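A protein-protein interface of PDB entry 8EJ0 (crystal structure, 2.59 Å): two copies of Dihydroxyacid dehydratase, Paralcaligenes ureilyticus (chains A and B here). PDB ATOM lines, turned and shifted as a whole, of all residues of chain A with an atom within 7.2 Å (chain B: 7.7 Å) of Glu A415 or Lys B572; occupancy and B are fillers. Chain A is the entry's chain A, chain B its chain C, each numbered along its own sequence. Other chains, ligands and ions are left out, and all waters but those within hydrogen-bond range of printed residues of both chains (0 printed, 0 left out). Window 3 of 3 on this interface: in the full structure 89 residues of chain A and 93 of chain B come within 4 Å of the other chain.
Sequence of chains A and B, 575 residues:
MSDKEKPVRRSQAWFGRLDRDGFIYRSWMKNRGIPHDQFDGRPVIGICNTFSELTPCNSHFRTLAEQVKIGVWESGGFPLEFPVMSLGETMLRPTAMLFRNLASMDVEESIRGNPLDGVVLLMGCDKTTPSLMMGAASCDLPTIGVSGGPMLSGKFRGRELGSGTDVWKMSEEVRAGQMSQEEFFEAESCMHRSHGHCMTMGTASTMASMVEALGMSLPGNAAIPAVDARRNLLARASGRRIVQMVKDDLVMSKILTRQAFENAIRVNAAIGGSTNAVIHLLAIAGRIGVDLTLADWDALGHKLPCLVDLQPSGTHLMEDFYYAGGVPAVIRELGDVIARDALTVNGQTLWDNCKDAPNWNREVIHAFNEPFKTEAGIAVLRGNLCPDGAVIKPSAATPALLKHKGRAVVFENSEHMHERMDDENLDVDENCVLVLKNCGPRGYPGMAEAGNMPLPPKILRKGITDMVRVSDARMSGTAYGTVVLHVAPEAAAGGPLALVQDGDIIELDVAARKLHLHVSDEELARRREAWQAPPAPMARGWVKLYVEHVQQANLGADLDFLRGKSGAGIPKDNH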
ATOM      1  N   LEU A  92      23.468 -12.648  35.483  1.00  0.00           N
ATOM      2  CA  LEU A  92      22.732 -11.431  35.798  1.00  0.00           C
ATOM      3  C   LEU A  92      23.251 -10.259  34.974  1.00  0.00           C
ATOM      4  O   LEU A  92      24.445  -9.943  35.004  1.00  0.00           O
ATOM      5  CB  LEU A  92      22.827 -11.122  37.289  1.00  0.00           C
ATOM      6  CG  LEU A  92      21.784 -11.825  38.158  1.00  0.00           C
ATOM      7  CD1 LEU A  92      21.941 -11.418  39.609  1.00  0.00           C
ATOM      8  CD2 LEU A  92      20.381 -11.508  37.662  1.00  0.00           C
ATOM      9  N   ARG A  93      22.346  -9.614  34.241  1.00  0.00           N
ATOM     10  CA  ARG A  93      22.618  -8.435  33.439  1.00  0.00           C
ATOM     11  C   ARG A  93      21.667  -7.309  33.836  1.00  0.00           C
ATOM     12  O   ARG A  93      20.539  -7.575  34.261  1.00  0.00           O
ATOM     13  CB  ARG A  93      22.470  -8.746  31.944  1.00  0.00           C
ATOM     14  CG  ARG A  93      23.581  -9.630  31.401  1.00  0.00           C
ATOM     15  CD  ARG A  93      23.240 -10.197  30.035  1.00  0.00           C
ATOM     16  NE  ARG A  93      22.907  -9.167  29.059  1.00  0.00           N
ATOM     17  CZ  ARG A  93      22.637  -9.414  27.781  1.00  0.00           C
ATOM     18  NH1 ARG A  93      22.661 -10.659  27.325  1.00  0.00           N
ATOM     19  NH2 ARG A  93      22.342  -8.417  26.958  1.00  0.00           N
ATOM     20  N   PRO A  94      22.086  -6.035  33.713  1.00  0.00           N
ATOM     21  CA  PRO A  94      23.327  -5.477  33.154  1.00  0.00           C
ATOM     22  C   PRO A  94      24.600  -5.898  33.881  1.00  0.00           C
ATOM     23  O   PRO A  94      25.659  -5.908  33.262  1.00  0.00           O
ATOM     24  CB  PRO A  94      23.125  -3.962  33.294  1.00  0.00           C
ATOM     25  CG  PRO A  94      21.661  -3.774  33.435  1.00  0.00           C
ATOM     26  CD  PRO A  94      21.186  -4.971  34.186  1.00  0.00           C
ATOM     27  N   THR A  95      24.494  -6.224  35.166  1.00  0.00           N
ATOM     28  CA  THR A  95      25.616  -6.714  35.956  1.00  0.00           C
ATOM     29  C   THR A  95      25.088  -7.147  37.315  1.00  0.00           C
ATOM     30  O   THR A  95      24.071  -6.633  37.789  1.00  0.00           O
ATOM     31  CB  THR A  95      26.716  -5.653  36.121  1.00  0.00           C
ATOM     32  OG1 THR A  95      27.818  -6.208  36.850  1.00  0.00           O
ATOM     33  CG2 THR A  95      26.186  -4.433  36.857  1.00  0.00           C
ATOM     34  N   PHE A 411      35.360   7.552  24.925  1.00  0.00           N
ATOM     35  CA  PHE A 411      34.129   6.837  24.607  1.00  0.00           C
ATOM     36  C   PHE A 411      33.057   7.286  25.589  1.00  0.00           C
ATOM     37  O   PHE A 411      33.245   7.182  26.807  1.00  0.00           O
ATOM     38  CB  PHE A 411      34.337   5.323  24.679  1.00  0.00           C
ATOM     39  CG  PHE A 411      35.512   4.837  23.880  1.00  0.00           C
ATOM     40  CD1 PHE A 411      35.419   4.691  22.506  1.00  0.00           C
ATOM     41  CD2 PHE A 411      36.712   4.535  24.502  1.00  0.00           C
ATOM     42  CE1 PHE A 411      36.499   4.249  21.767  1.00  0.00           C
ATOM     43  CE2 PHE A 411      37.797   4.091  23.768  1.00  0.00           C
ATOM     44  CZ  PHE A 411      37.689   3.950  22.398  1.00  0.00           C
ATOM     45  N   GLU A 412      31.938   7.790  25.063  1.00  0.00           N
ATOM     46  CA  GLU A 412      30.914   8.366  25.928  1.00  0.00           C
ATOM     47  C   GLU A 412      30.162   7.301  26.716  1.00  0.00           C
ATOM     48  O   GLU A 412      29.643   7.589  27.800  1.00  0.00           O
ATOM     49  CB  GLU A 412      29.940   9.207  25.103  1.00  0.00           C
ATOM     50  CG  GLU A 412      30.547  10.484  24.541  1.00  0.00           C
ATOM     51  CD  GLU A 412      31.187  11.345  25.614  1.00  0.00           C
ATOM     52  OE1 GLU A 412      32.317  11.832  25.394  1.00  0.00           O
ATOM     53  OE2 GLU A 412      30.565  11.529  26.681  1.00  0.00           O
ATOM     54  N   ASN A 413      30.087   6.078  26.198  1.00  0.00           N
ATOM     55  CA  ASN A 413      29.438   4.981  26.903  1.00  0.00           C
ATOM     56  C   ASN A 413      29.959   3.666  26.336  1.00  0.00           C
ATOM     57  O   ASN A 413      30.826   3.643  25.460  1.00  0.00           O
ATOM     58  CB  ASN A 413      27.913   5.074  26.802  1.00  0.00           C
ATOM     59  CG  ASN A 413      27.432   5.299  25.383  1.00  0.00           C
ATOM     60  OD1 ASN A 413      27.533   4.418  24.530  1.00  0.00           O
ATOM     61  ND2 ASN A 413      26.895   6.486  25.124  1.00  0.00           N
ATOM     62  N   SER A 414      29.417   2.561  26.854  1.00  0.00           N
ATOM     63  CA  SER A 414      29.872   1.241  26.427  1.00  0.00           C
ATOM     64  C   SER A 414      29.470   0.951  24.986  1.00  0.00           C
ATOM     65  O   SER A 414      30.268   0.408  24.212  1.00  0.00           O
ATOM     66  CB  SER A 414      29.322   0.170  27.368  1.00  0.00           C
ATOM     67  OG  SER A 414      27.919   0.297  27.522  1.00  0.00           O
ATOM     68  N   GLU A 415      28.237   1.298  24.607  1.00  0.00           N
ATOM     69  CA  GLU A 415      27.804   1.106  23.226  1.00  0.00           C
ATOM     70  C   GLU A 415      28.693   1.887  22.268  1.00  0.00           C
ATOM     71  O   GLU A 415      29.126   1.364  21.236  1.00  0.00           O
ATOM     72  CB  GLU A 415      26.343   1.532  23.061  1.00  0.00           C
ATOM     73  CG  GLU A 415      25.390   1.000  24.118  1.00  0.00           C
ATOM     74  CD  GLU A 415      25.302   1.903  25.336  1.00  0.00           C
ATOM     75  OE1 GLU A 415      26.360   2.229  25.915  1.00  0.00           O
ATOM     76  OE2 GLU A 415      24.175   2.292  25.708  1.00  0.00           O
ATOM     77  N   HIS A 416      28.980   3.147  22.604  1.00  0.00           N
ATOM     78  CA  HIS A 416      29.847   3.966  21.766  1.00  0.00           C
ATOM     79  C   HIS A 416      31.260   3.403  21.703  1.00  0.00           C
ATOM     80  O   HIS A 416      31.970   3.620  20.715  1.00  0.00           O
ATOM     81  CB  HIS A 416      29.863   5.402  22.288  1.00  0.00           C
ATOM     82  CG  HIS A 416      30.677   6.343  21.459  1.00  0.00           C
ATOM     83  ND1 HIS A 416      31.761   7.031  21.960  1.00  0.00           N
ATOM     84  CD2 HIS A 416      30.564   6.714  20.161  1.00  0.00           C
ATOM     85  CE1 HIS A 416      32.280   7.784  21.007  1.00  0.00           C
ATOM     86  NE2 HIS A 416      31.572   7.611  19.906  1.00  0.00           N
ATOM     87  N   MET A 417      31.685   2.677  22.740  1.00  0.00           N
ATOM     88  CA  MET A 417      33.013   2.074  22.720  1.00  0.00           C
ATOM     89  C   MET A 417      33.081   0.934  21.713  1.00  0.00           C
ATOM     90  O   MET A 417      33.973   0.901  20.858  1.00  0.00           O
ATOM     91  CB  MET A 417      33.392   1.579  24.116  1.00  0.00           C
ATOM     92  CG  MET A 417      34.835   1.113  24.220  1.00  0.00           C
ATOM     93  SD  MET A 417      35.174   0.156  25.707  1.00  0.00           S
ATOM     94  CE  MET A 417      34.222  -1.323  25.376  1.00  0.00           C
ATOM     95  N   HIS A 418      32.138  -0.011  21.795  1.00  0.00           N
ATOM     96  CA  HIS A 418      32.129  -1.138  20.867  1.00  0.00           C
ATOM     97  C   HIS A 418      32.006  -0.678  19.420  1.00  0.00           C
ATOM     98  O   HIS A 418      32.480  -1.363  18.508  1.00  0.00           O
ATOM     99  CB  HIS A 418      30.986  -2.096  21.214  1.00  0.00           C
ATOM    100  CG  HIS A 418      31.065  -2.655  22.602  1.00  0.00           C
ATOM    101  ND1 HIS A 418      29.964  -2.766  23.422  1.00  0.00           N
ATOM    102  CD2 HIS A 418      32.112  -3.139  23.310  1.00  0.00           C
ATOM    103  CE1 HIS A 418      30.329  -3.291  24.579  1.00  0.00           C
ATOM    104  NE2 HIS A 418      31.629  -3.526  24.536  1.00  0.00           N
ATOM    105  N   GLU A 419      31.381   0.479  19.192  1.00  0.00           N
ATOM    106  CA  GLU A 419      31.235   0.988  17.832  1.00  0.00           C
ATOM    107  C   GLU A 419      32.557   1.529  17.299  1.00  0.00           C
ATOM    108  O   GLU A 419      32.974   1.189  16.186  1.00  0.00           O
ATOM    109  CB  GLU A 419      30.155   2.070  17.792  1.00  0.00           C
ATOM    110  CG  GLU A 419      28.754   1.565  18.091  1.00  0.00           C
ATOM    111  CD  GLU A 419      27.748   2.690  18.245  1.00  0.00           C
ATOM    112  OE1 GLU A 419      26.540   2.396  18.370  1.00  0.00           O
ATOM    113  OE2 GLU A 419      28.164   3.868  18.241  1.00  0.00           O
ATOM    114  N   ARG A 420      33.236   2.369  18.083  1.00  0.00           N
ATOM    115  CA  ARG A 420      34.440   3.042  17.613  1.00  0.00           C
ATOM    116  C   ARG A 420      35.720   2.254  17.851  1.00  0.00           C
ATOM    117  O   ARG A 420      36.724   2.526  17.183  1.00  0.00           O
ATOM    118  CB  ARG A 420      34.575   4.417  18.278  1.00  0.00           C
ATOM    119  CG  ARG A 420      34.062   5.571  17.433  1.00  0.00           C
ATOM    120  CD  ARG A 420      34.199   6.902  18.157  1.00  0.00           C
ATOM    121  NE  ARG A 420      35.590   7.256  18.432  1.00  0.00           N
ATOM    122  CZ  ARG A 420      35.963   8.362  19.068  1.00  0.00           C
ATOM    123  NH1 ARG A 420      35.050   9.222  19.497  1.00  0.00           N
ATOM    124  NH2 ARG A 420      37.250   8.608  19.276  1.00  0.00           N
ATOM    125  N   MET A 421      35.719   1.292  18.780  1.00  0.00           N
ATOM    126  CA  MET A 421      36.960   0.597  19.116  1.00  0.00           C
ATOM    127  C   MET A 421      37.505  -0.183  17.926  1.00  0.00           C
ATOM    128  O   MET A 421      38.709  -0.145  17.651  1.00  0.00           O
ATOM    129  CB  MET A 421      36.742  -0.336  20.307  1.00  0.00           C
ATOM    130  CG  MET A 421      38.021  -0.962  20.834  1.00  0.00           C
ATOM    131  SD  MET A 421      39.120   0.251  21.589  1.00  0.00           S
ATOM    132  CE  MET A 421      38.265   0.570  23.128  1.00  0.00           C
ATOM    133  N   LEU A 436      36.607   5.714  29.158  1.00  0.00           N
ATOM    134  CA  LEU A 436      35.243   5.211  29.070  1.00  0.00           C
ATOM    135  C   LEU A 436      34.385   5.902  30.120  1.00  0.00           C
ATOM    136  O   LEU A 436      34.726   5.893  31.307  1.00  0.00           O
ATOM    137  CB  LEU A 436      35.207   3.694  29.265  1.00  0.00           C
ATOM    138  CG  LEU A 436      33.836   3.037  29.436  1.00  0.00           C
ATOM    139  CD1 LEU A 436      32.986   3.222  28.189  1.00  0.00           C
ATOM    140  CD2 LEU A 436      33.993   1.563  29.771  1.00  0.00           C
ATOM    141  N   LYS A 437      33.276   6.492  29.684  1.00  0.00           N
ATOM    142  CA  LYS A 437      32.401   7.269  30.546  1.00  0.00           C
ATOM    143  C   LYS A 437      31.094   6.533  30.813  1.00  0.00           C
ATOM    144  O   LYS A 437      30.682   5.649  30.058  1.00  0.00           O
ATOM    145  CB  LYS A 437      32.082   8.633  29.926  1.00  0.00           C
ATOM    146  CG  LYS A 437      33.266   9.553  29.705  1.00  0.00           C
ATOM    147  CD  LYS A 437      32.803  10.820  28.999  1.00  0.00           C
ATOM    148  CE  LYS A 437      33.947  11.780  28.737  1.00  0.00           C
ATOM    149  NZ  LYS A 437      33.514  12.925  27.888  1.00  0.00           N
ATOM    150  N   ASN A 438      30.448   6.926  31.913  1.00  0.00           N
ATOM    151  CA  ASN A 438      29.063   6.553  32.211  1.00  0.00           C
ATOM    152  C   ASN A 438      28.898   5.045  32.384  1.00  0.00           C
ATOM    153  O   ASN A 438      27.950   4.442  31.875  1.00  0.00           O
ATOM    154  CB  ASN A 438      28.109   7.081  31.139  1.00  0.00           C
ATOM    155  CG  ASN A 438      28.172   8.589  31.004  1.00  0.00           C
ATOM    156  OD1 ASN A 438      27.667   9.321  31.855  1.00  0.00           O
ATOM    157  ND2 ASN A 438      28.795   9.062  29.931  1.00  0.00           N
ATOM    158  N   CYS A 439      29.821   4.425  33.122  1.00  0.00           N
ATOM    159  CA  CYS A 439      29.716   3.008  33.444  1.00  0.00           C
ATOM    160  C   CYS A 439      29.855   2.758  34.941  1.00  0.00           C
ATOM    161  O   CYS A 439      30.221   1.649  35.348  1.00  0.00           O
ATOM    162  CB  CYS A 439      30.752   2.194  32.666  1.00  0.00           C
ATOM    163  SG  CYS A 439      30.508   2.204  30.876  1.00  0.00           S
ATOM    164  N   GLY A 443      25.522   5.270  35.990  1.00  0.00           N
ATOM    165  CA  GLY A 443      25.538   5.382  34.537  1.00  0.00           C
ATOM    166  C   GLY A 443      25.117   4.120  33.806  1.00  0.00           C
ATOM    167  O   GLY A 443      24.316   4.180  32.866  1.00  0.00           O
ATOM    168  N   TYR A 444      25.646   2.965  34.221  1.00  0.00           N
ATOM    169  CA  TYR A 444      25.451   1.747  33.434  1.00  0.00           C
ATOM    170  C   TYR A 444      23.994   1.296  33.393  1.00  0.00           C
ATOM    171  O   TYR A 444      23.480   1.058  32.287  1.00  0.00           O
ATOM    172  CB  TYR A 444      26.375   0.642  33.954  1.00  0.00           C
ATOM    173  CG  TYR A 444      26.705  -0.404  32.916  1.00  0.00           C
ATOM    174  CD1 TYR A 444      27.751  -0.212  32.027  1.00  0.00           C
ATOM    175  CD2 TYR A 444      25.972  -1.581  32.823  1.00  0.00           C
ATOM    176  CE1 TYR A 444      28.062  -1.161  31.078  1.00  0.00           C
ATOM    177  CE2 TYR A 444      26.279  -2.536  31.875  1.00  0.00           C
ATOM    178  CZ  TYR A 444      27.322  -2.323  31.006  1.00  0.00           C
ATOM    179  OH  TYR A 444      27.622  -3.279  30.066  1.00  0.00           O
ATOM    180  N   PRO A 445      23.271   1.151  34.521  1.00  0.00           N
ATOM    181  CA  PRO A 445      23.637   1.295  35.937  1.00  0.00           C
ATOM    182  C   PRO A 445      24.119  -0.018  36.553  1.00  0.00           C
ATOM    183  O   PRO A 445      23.927  -1.084  35.964  1.00  0.00           O
ATOM    184  CB  PRO A 445      22.324   1.744  36.577  1.00  0.00           C
ATOM    185  CG  PRO A 445      21.295   1.010  35.788  1.00  0.00           C
ATOM    186  CD  PRO A 445      21.826   0.916  34.369  1.00  0.00           C
ATOM    187  N   ALA A 448      29.307  -1.958  35.819  1.00  0.00           N
ATOM    188  CA  ALA A 448      29.667  -3.242  35.255  1.00  0.00           C
ATOM    189  C   ALA A 448      31.179  -3.361  35.105  1.00  0.00           C
ATOM    190  O   ALA A 448      31.931  -2.393  35.244  1.00  0.00           O
ATOM    191  CB  ALA A 448      28.979  -3.439  33.904  1.00  0.00           C
ATOM    192  N   TRP B  14      21.429 -14.317  25.480  1.00  0.00           N
ATOM    193  CA  TRP B  14      22.511 -14.813  26.328  1.00  0.00           C
ATOM    194  C   TRP B  14      23.220 -15.970  25.633  1.00  0.00           C
ATOM    195  O   TRP B  14      24.376 -15.853  25.220  1.00  0.00           O
ATOM    196  CB  TRP B  14      21.978 -15.302  27.676  1.00  0.00           C
ATOM    197  CG  TRP B  14      21.747 -14.271  28.739  1.00  0.00           C
ATOM    198  CD1 TRP B  14      22.534 -14.028  29.825  1.00  0.00           C
ATOM    199  CD2 TRP B  14      20.622 -13.391  28.854  1.00  0.00           C
ATOM    200  NE1 TRP B  14      21.983 -13.038  30.599  1.00  0.00           N
ATOM    201  CE2 TRP B  14      20.809 -12.628  30.023  1.00  0.00           C
ATOM    202  CE3 TRP B  14      19.482 -13.169  28.078  1.00  0.00           C
ATOM    203  CZ2 TRP B  14      19.900 -11.653  30.431  1.00  0.00           C
ATOM    204  CZ3 TRP B  14      18.579 -12.202  28.484  1.00  0.00           C
ATOM    205  CH2 TRP B  14      18.794 -11.457  29.650  1.00  0.00           C
ATOM    206  N   ARG B  17      24.657 -16.217  21.676  1.00  0.00           N
ATOM    207  CA  ARG B  17      25.666 -15.258  21.254  1.00  0.00           C
ATOM    208  C   ARG B  17      26.930 -15.959  20.775  1.00  0.00           C
ATOM    209  O   ARG B  17      27.402 -16.917  21.396  1.00  0.00           O
ATOM    210  CB  ARG B  17      26.008 -14.310  22.401  1.00  0.00           C
ATOM    211  CG  ARG B  17      24.824 -13.539  22.943  1.00  0.00           C
ATOM    212  CD  ARG B  17      24.501 -12.335  22.077  1.00  0.00           C
ATOM    213  NE  ARG B  17      25.551 -11.324  22.149  1.00  0.00           N
ATOM    214  CZ  ARG B  17      25.656 -10.424  23.120  1.00  0.00           C
ATOM    215  NH1 ARG B  17      24.772 -10.408  24.110  1.00  0.00           N
ATOM    216  NH2 ARG B  17      26.645  -9.540  23.106  1.00  0.00           N
ATOM    217  N   ASP B  21      31.059 -12.608  24.780  1.00  0.00           N
ATOM    218  CA  ASP B  21      30.038 -12.773  25.806  1.00  0.00           C
ATOM    219  C   ASP B  21      29.343 -14.123  25.701  1.00  0.00           C
ATOM    220  O   ASP B  21      28.902 -14.669  26.718  1.00  0.00           O
ATOM    221  CB  ASP B  21      29.018 -11.637  25.708  1.00  0.00           C
ATOM    222  CG  ASP B  21      29.670 -10.268  25.736  1.00  0.00           C
ATOM    223  OD1 ASP B  21      30.621 -10.080  26.525  1.00  0.00           O
ATOM    224  OD2 ASP B  21      29.237  -9.382  24.971  1.00  0.00           O
ATOM    225  N   TYR B  25      28.472 -16.485  28.753  1.00  0.00           N
ATOM    226  CA  TYR B  25      27.111 -16.871  29.105  1.00  0.00           C
ATOM    227  C   TYR B  25      26.896 -18.380  29.130  1.00  0.00           C
ATOM    228  O   TYR B  25      25.888 -18.830  29.686  1.00  0.00           O
ATOM    229  CB  TYR B  25      26.120 -16.228  28.130  1.00  0.00           C
ATOM    230  CG  TYR B  25      26.088 -14.718  28.206  1.00  0.00           C
ATOM    231  CD1 TYR B  25      26.264 -14.063  29.416  1.00  0.00           C
ATOM    232  CD2 TYR B  25      25.892 -13.946  27.068  1.00  0.00           C
ATOM    233  CE1 TYR B  25      26.239 -12.684  29.494  1.00  0.00           C
ATOM    234  CE2 TYR B  25      25.865 -12.567  27.134  1.00  0.00           C
ATOM    235  CZ  TYR B  25      26.039 -11.940  28.350  1.00  0.00           C
ATOM    236  OH  TYR B  25      26.015 -10.566  28.416  1.00  0.00           O
ATOM    237  N   GLY B 113      16.817 -10.115  34.910  1.00  0.00           N
ATOM    238  CA  GLY B 113      18.263 -10.168  34.824  1.00  0.00           C
ATOM    239  C   GLY B 113      18.844 -11.472  34.323  1.00  0.00           C
ATOM    240  O   GLY B 113      20.036 -11.513  34.002  1.00  0.00           O
ATOM    241  N   GLY B 569      12.592  -6.777  28.460  1.00  0.00           N
ATOM    242  CA  GLY B 569      13.561  -6.453  27.434  1.00  0.00           C
ATOM    243  C   GLY B 569      14.941  -6.981  27.777  1.00  0.00           C
ATOM    244  O   GLY B 569      15.241  -7.376  28.904  1.00  0.00           O
ATOM    245  N   ILE B 570      15.804  -6.988  26.765  1.00  0.00           N
ATOM    246  CA  ILE B 570      17.158  -7.515  26.892  1.00  0.00           C
ATOM    247  C   ILE B 570      18.058  -6.380  27.375  1.00  0.00           C
ATOM    248  O   ILE B 570      18.263  -5.410  26.626  1.00  0.00           O
ATOM    249  CB  ILE B 570      17.662  -8.094  25.565  1.00  0.00           C
ATOM    250  CG1 ILE B 570      16.675  -9.138  25.038  1.00  0.00           C
ATOM    251  CG2 ILE B 570      19.045  -8.693  25.750  1.00  0.00           C
ATOM    252  CD1 ILE B 570      16.346  -8.985  23.567  1.00  0.00           C
ATOM    253  N   PRO B 571      18.606  -6.454  28.589  1.00  0.00           N
ATOM    254  CA  PRO B 571      19.458  -5.363  29.079  1.00  0.00           C
ATOM    255  C   PRO B 571      20.855  -5.398  28.479  1.00  0.00           C
ATOM    256  O   PRO B 571      21.138  -6.203  27.585  1.00  0.00           O
ATOM    257  CB  PRO B 571      19.492  -5.607  30.591  1.00  0.00           C
ATOM    258  CG  PRO B 571      19.336  -7.086  30.722  1.00  0.00           C
ATOM    259  CD  PRO B 571      18.425  -7.515  29.596  1.00  0.00           C
ATOM    260  N   LYS B 572      21.732  -4.524  28.967  1.00  0.00           N
ATOM    261  CA  LYS B 572      23.114  -4.499  28.513  1.00  0.00           C
ATOM    262  C   LYS B 572      23.827  -5.796  28.886  1.00  0.00           C
ATOM    263  O   LYS B 572      23.381  -6.563  29.744  1.00  0.00           O
ATOM    264  CB  LYS B 572      23.864  -3.319  29.129  1.00  0.00           C
ATOM    265  CG  LYS B 572      23.464  -1.949  28.615  1.00  0.00           C
ATOM    266  CD  LYS B 572      23.902  -0.874  29.601  1.00  0.00           C
ATOM    267  CE  LYS B 572      24.045   0.484  28.938  1.00  0.00           C
ATOM    268  NZ  LYS B 572      25.294   0.567  28.133  1.00  0.00           N
ATOM    269  N   ASP B 573      24.958  -6.033  28.229  1.00  0.00           N
ATOM    270  CA  ASP B 573      25.833  -7.122  28.623  1.00  0.00           C
ATOM    271  C   ASP B 573      26.580  -6.752  29.903  1.00  0.00           C
ATOM    272  O   ASP B 573      26.665  -5.583  30.289  1.00  0.00           O
ATOM    273  CB  ASP B 573      26.817  -7.449  27.499  1.00  0.00           C
ATOM    274  CG  ASP B 573      26.131  -8.030  26.279  1.00  0.00           C
ATOM    275  OD1 ASP B 573      25.685  -9.195  26.345  1.00  0.00           O
ATOM    276  OD2 ASP B 573      26.022  -7.317  25.260  1.00  0.00           O
ATOM    277  N   ASN B 574      27.124  -7.767  30.568  1.00  0.00           N
ATOM    278  CA  ASN B 574      27.772  -7.570  31.858  1.00  0.00           C
ATOM    279  C   ASN B 574      29.272  -7.335  31.753  1.00  0.00           C
ATOM    280  O   ASN B 574      29.933  -7.188  32.787  1.00  0.00           O
ATOM    281  CB  ASN B 574      27.492  -8.763  32.779  1.00  0.00           C
ATOM    282  CG  ASN B 574      27.509 -10.087  32.044  1.00  0.00           C
ATOM    283  OD1 ASN B 574      28.305 -10.292  31.128  1.00  0.00           O
ATOM    284  ND2 ASN B 574      26.621 -10.991  32.437  1.00  0.00           N
ATOM    285  N   HIS B 575      29.824  -7.286  30.544  1.00  0.00           N
ATOM    286  CA  HIS B 575      31.243  -6.994  30.362  1.00  0.00           C
ATOM    287  C   HIS B 575      31.474  -6.206  29.078  1.00  0.00           C
ATOM    288  O   HIS B 575      30.574  -6.076  28.249  1.00  0.00           O
ATOM    289  CB  HIS B 575      32.065  -8.286  30.343  1.00  0.00           C
ATOM    290  CG  HIS B 575      31.968  -9.084  31.606  1.00  0.00           C
ATOM    291  ND1 HIS B 575      30.953  -9.987  31.839  1.00  0.00           N
ATOM    292  CD2 HIS B 575      32.752  -9.107  32.709  1.00  0.00           C
ATOM    293  CE1 HIS B 575      31.119 -10.536  33.029  1.00  0.00           C
ATOM    294  NE2 HIS B 575      32.203 -10.020  33.578  1.00  0.00           N
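Among the printed residues, merely in contact across the chains: Pro A94 with Asn B574 (3.0 Å), Arg A93 with Trp B14 (3.2 Å), Leu A92 with Gly B113 (3.2 Å), Tyr A444 with Lys B572 (3.3 Å), Arg A93 with Asn B574 (3.5 Å), Arg A93 with Ile B570 (3.5 Å), Leu A92 with Asn B574 (3.5 Å), Pro A94 with Lys B572 (3.6 Å) and Arg A93 with Arg B17 (3.9 Å).
Of chain B, only Lys B572 (3.0 Å) comes within 4 Å of Glu A415. Lys B572 touches just these residues of chain A: Arg A93 (2.7 Å), Pro A94 (3.6 Å), Ser A414 (2.7 Å), Glu A415 (3.0 Å) and Tyr A444 (3.3 Å). Printed residues of chain A within 4 Å of Arg B17: Arg A93 (3.9 Å). Of the printed residues of chain A, Tyr B25 touches Arg A93. Printed residues of chain A within 4 Å of Ile B570: Arg A93. The nearest printed residue of chain B that does not touch Glu A415 is Asp B573 (8.2 Å).
No position is printed for both chains. Of the 18 pairs that touch across the chains among the printed residues, none has its exchanged pair printed and touching as well.
NE of Arg A93 sits close to OH of Tyr B25 (3.5 Å). The backbone NH (N) of Arg A93 lies within hydrogen-bond range of the backbone carbonyl oxygen (O) of Gly B113 (3.0 Å). The backbone carbonyl oxygen of Pro B571 is in hydrogen-bond range of the guanidinium group of Arg A93. The guanidinium group (NE) of Arg A93 lies within hydrogen-bond range of the backbone carbonyl oxygen (O) of Lys B572, at 2.7 Å. OD1 of Asp B573 is in salt-bridge range of NH2 of Arg A93. NZ of Lys B572 is in hydrogen-bond range of OG of Ser A414, at 2.7 Å. The side-chain carboxylate (OE1) of Glu A415 is in salt-bridge range of the side-chain amino group (NZ) of Lys B572, 3.0 Å away. OH of Tyr A444 is in hydrogen-bond range of O of Asp B573 (2.5 Å). O of Pro A94 lies close to O of Asp B573 (3.2 Å).
The side-chain carboxylate (OE1) of Glu A415 lies close to the side-chain amide oxygen (OD1) of Asn A413. OG of Ser A414 lies within hydrogen-bond range of OE1 of Glu A415, at 3.0 Å. The backbone carbonyl oxygen (O) of Ser A414 lies within hydrogen-bond range of a ring nitrogen (ND1) of His A418, 3.3 Å away. NH2 of Arg B17 is in salt-bridge range of OD2 of Asp B21, at 3.2 Å. OH of Tyr B25 lies within hydrogen-bond range of OD1 of Asp B573, at 2.5 Å. OD1 of Asn B574 sits at hydrogen-bond distance from ND1 of His B575 (2.8 Å).
Hydrophobic or aromatic side chains of chain B within 4 Å of the printed part of chain A: Trp B14, Tyr B25, Ile B570 and Pro B571. Of the 23 printed residues of chain A, 6 touch a printed residue of chain B. Printed residues of chain A that touch a printed residue of chain B: Leu A92, Arg A93, Pro A94, Ser A414, Glu A415 and Tyr A444. Hydrophobic or aromatic side chains of chain A that line the printed part of chain B: Leu A92 and Tyr A444.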
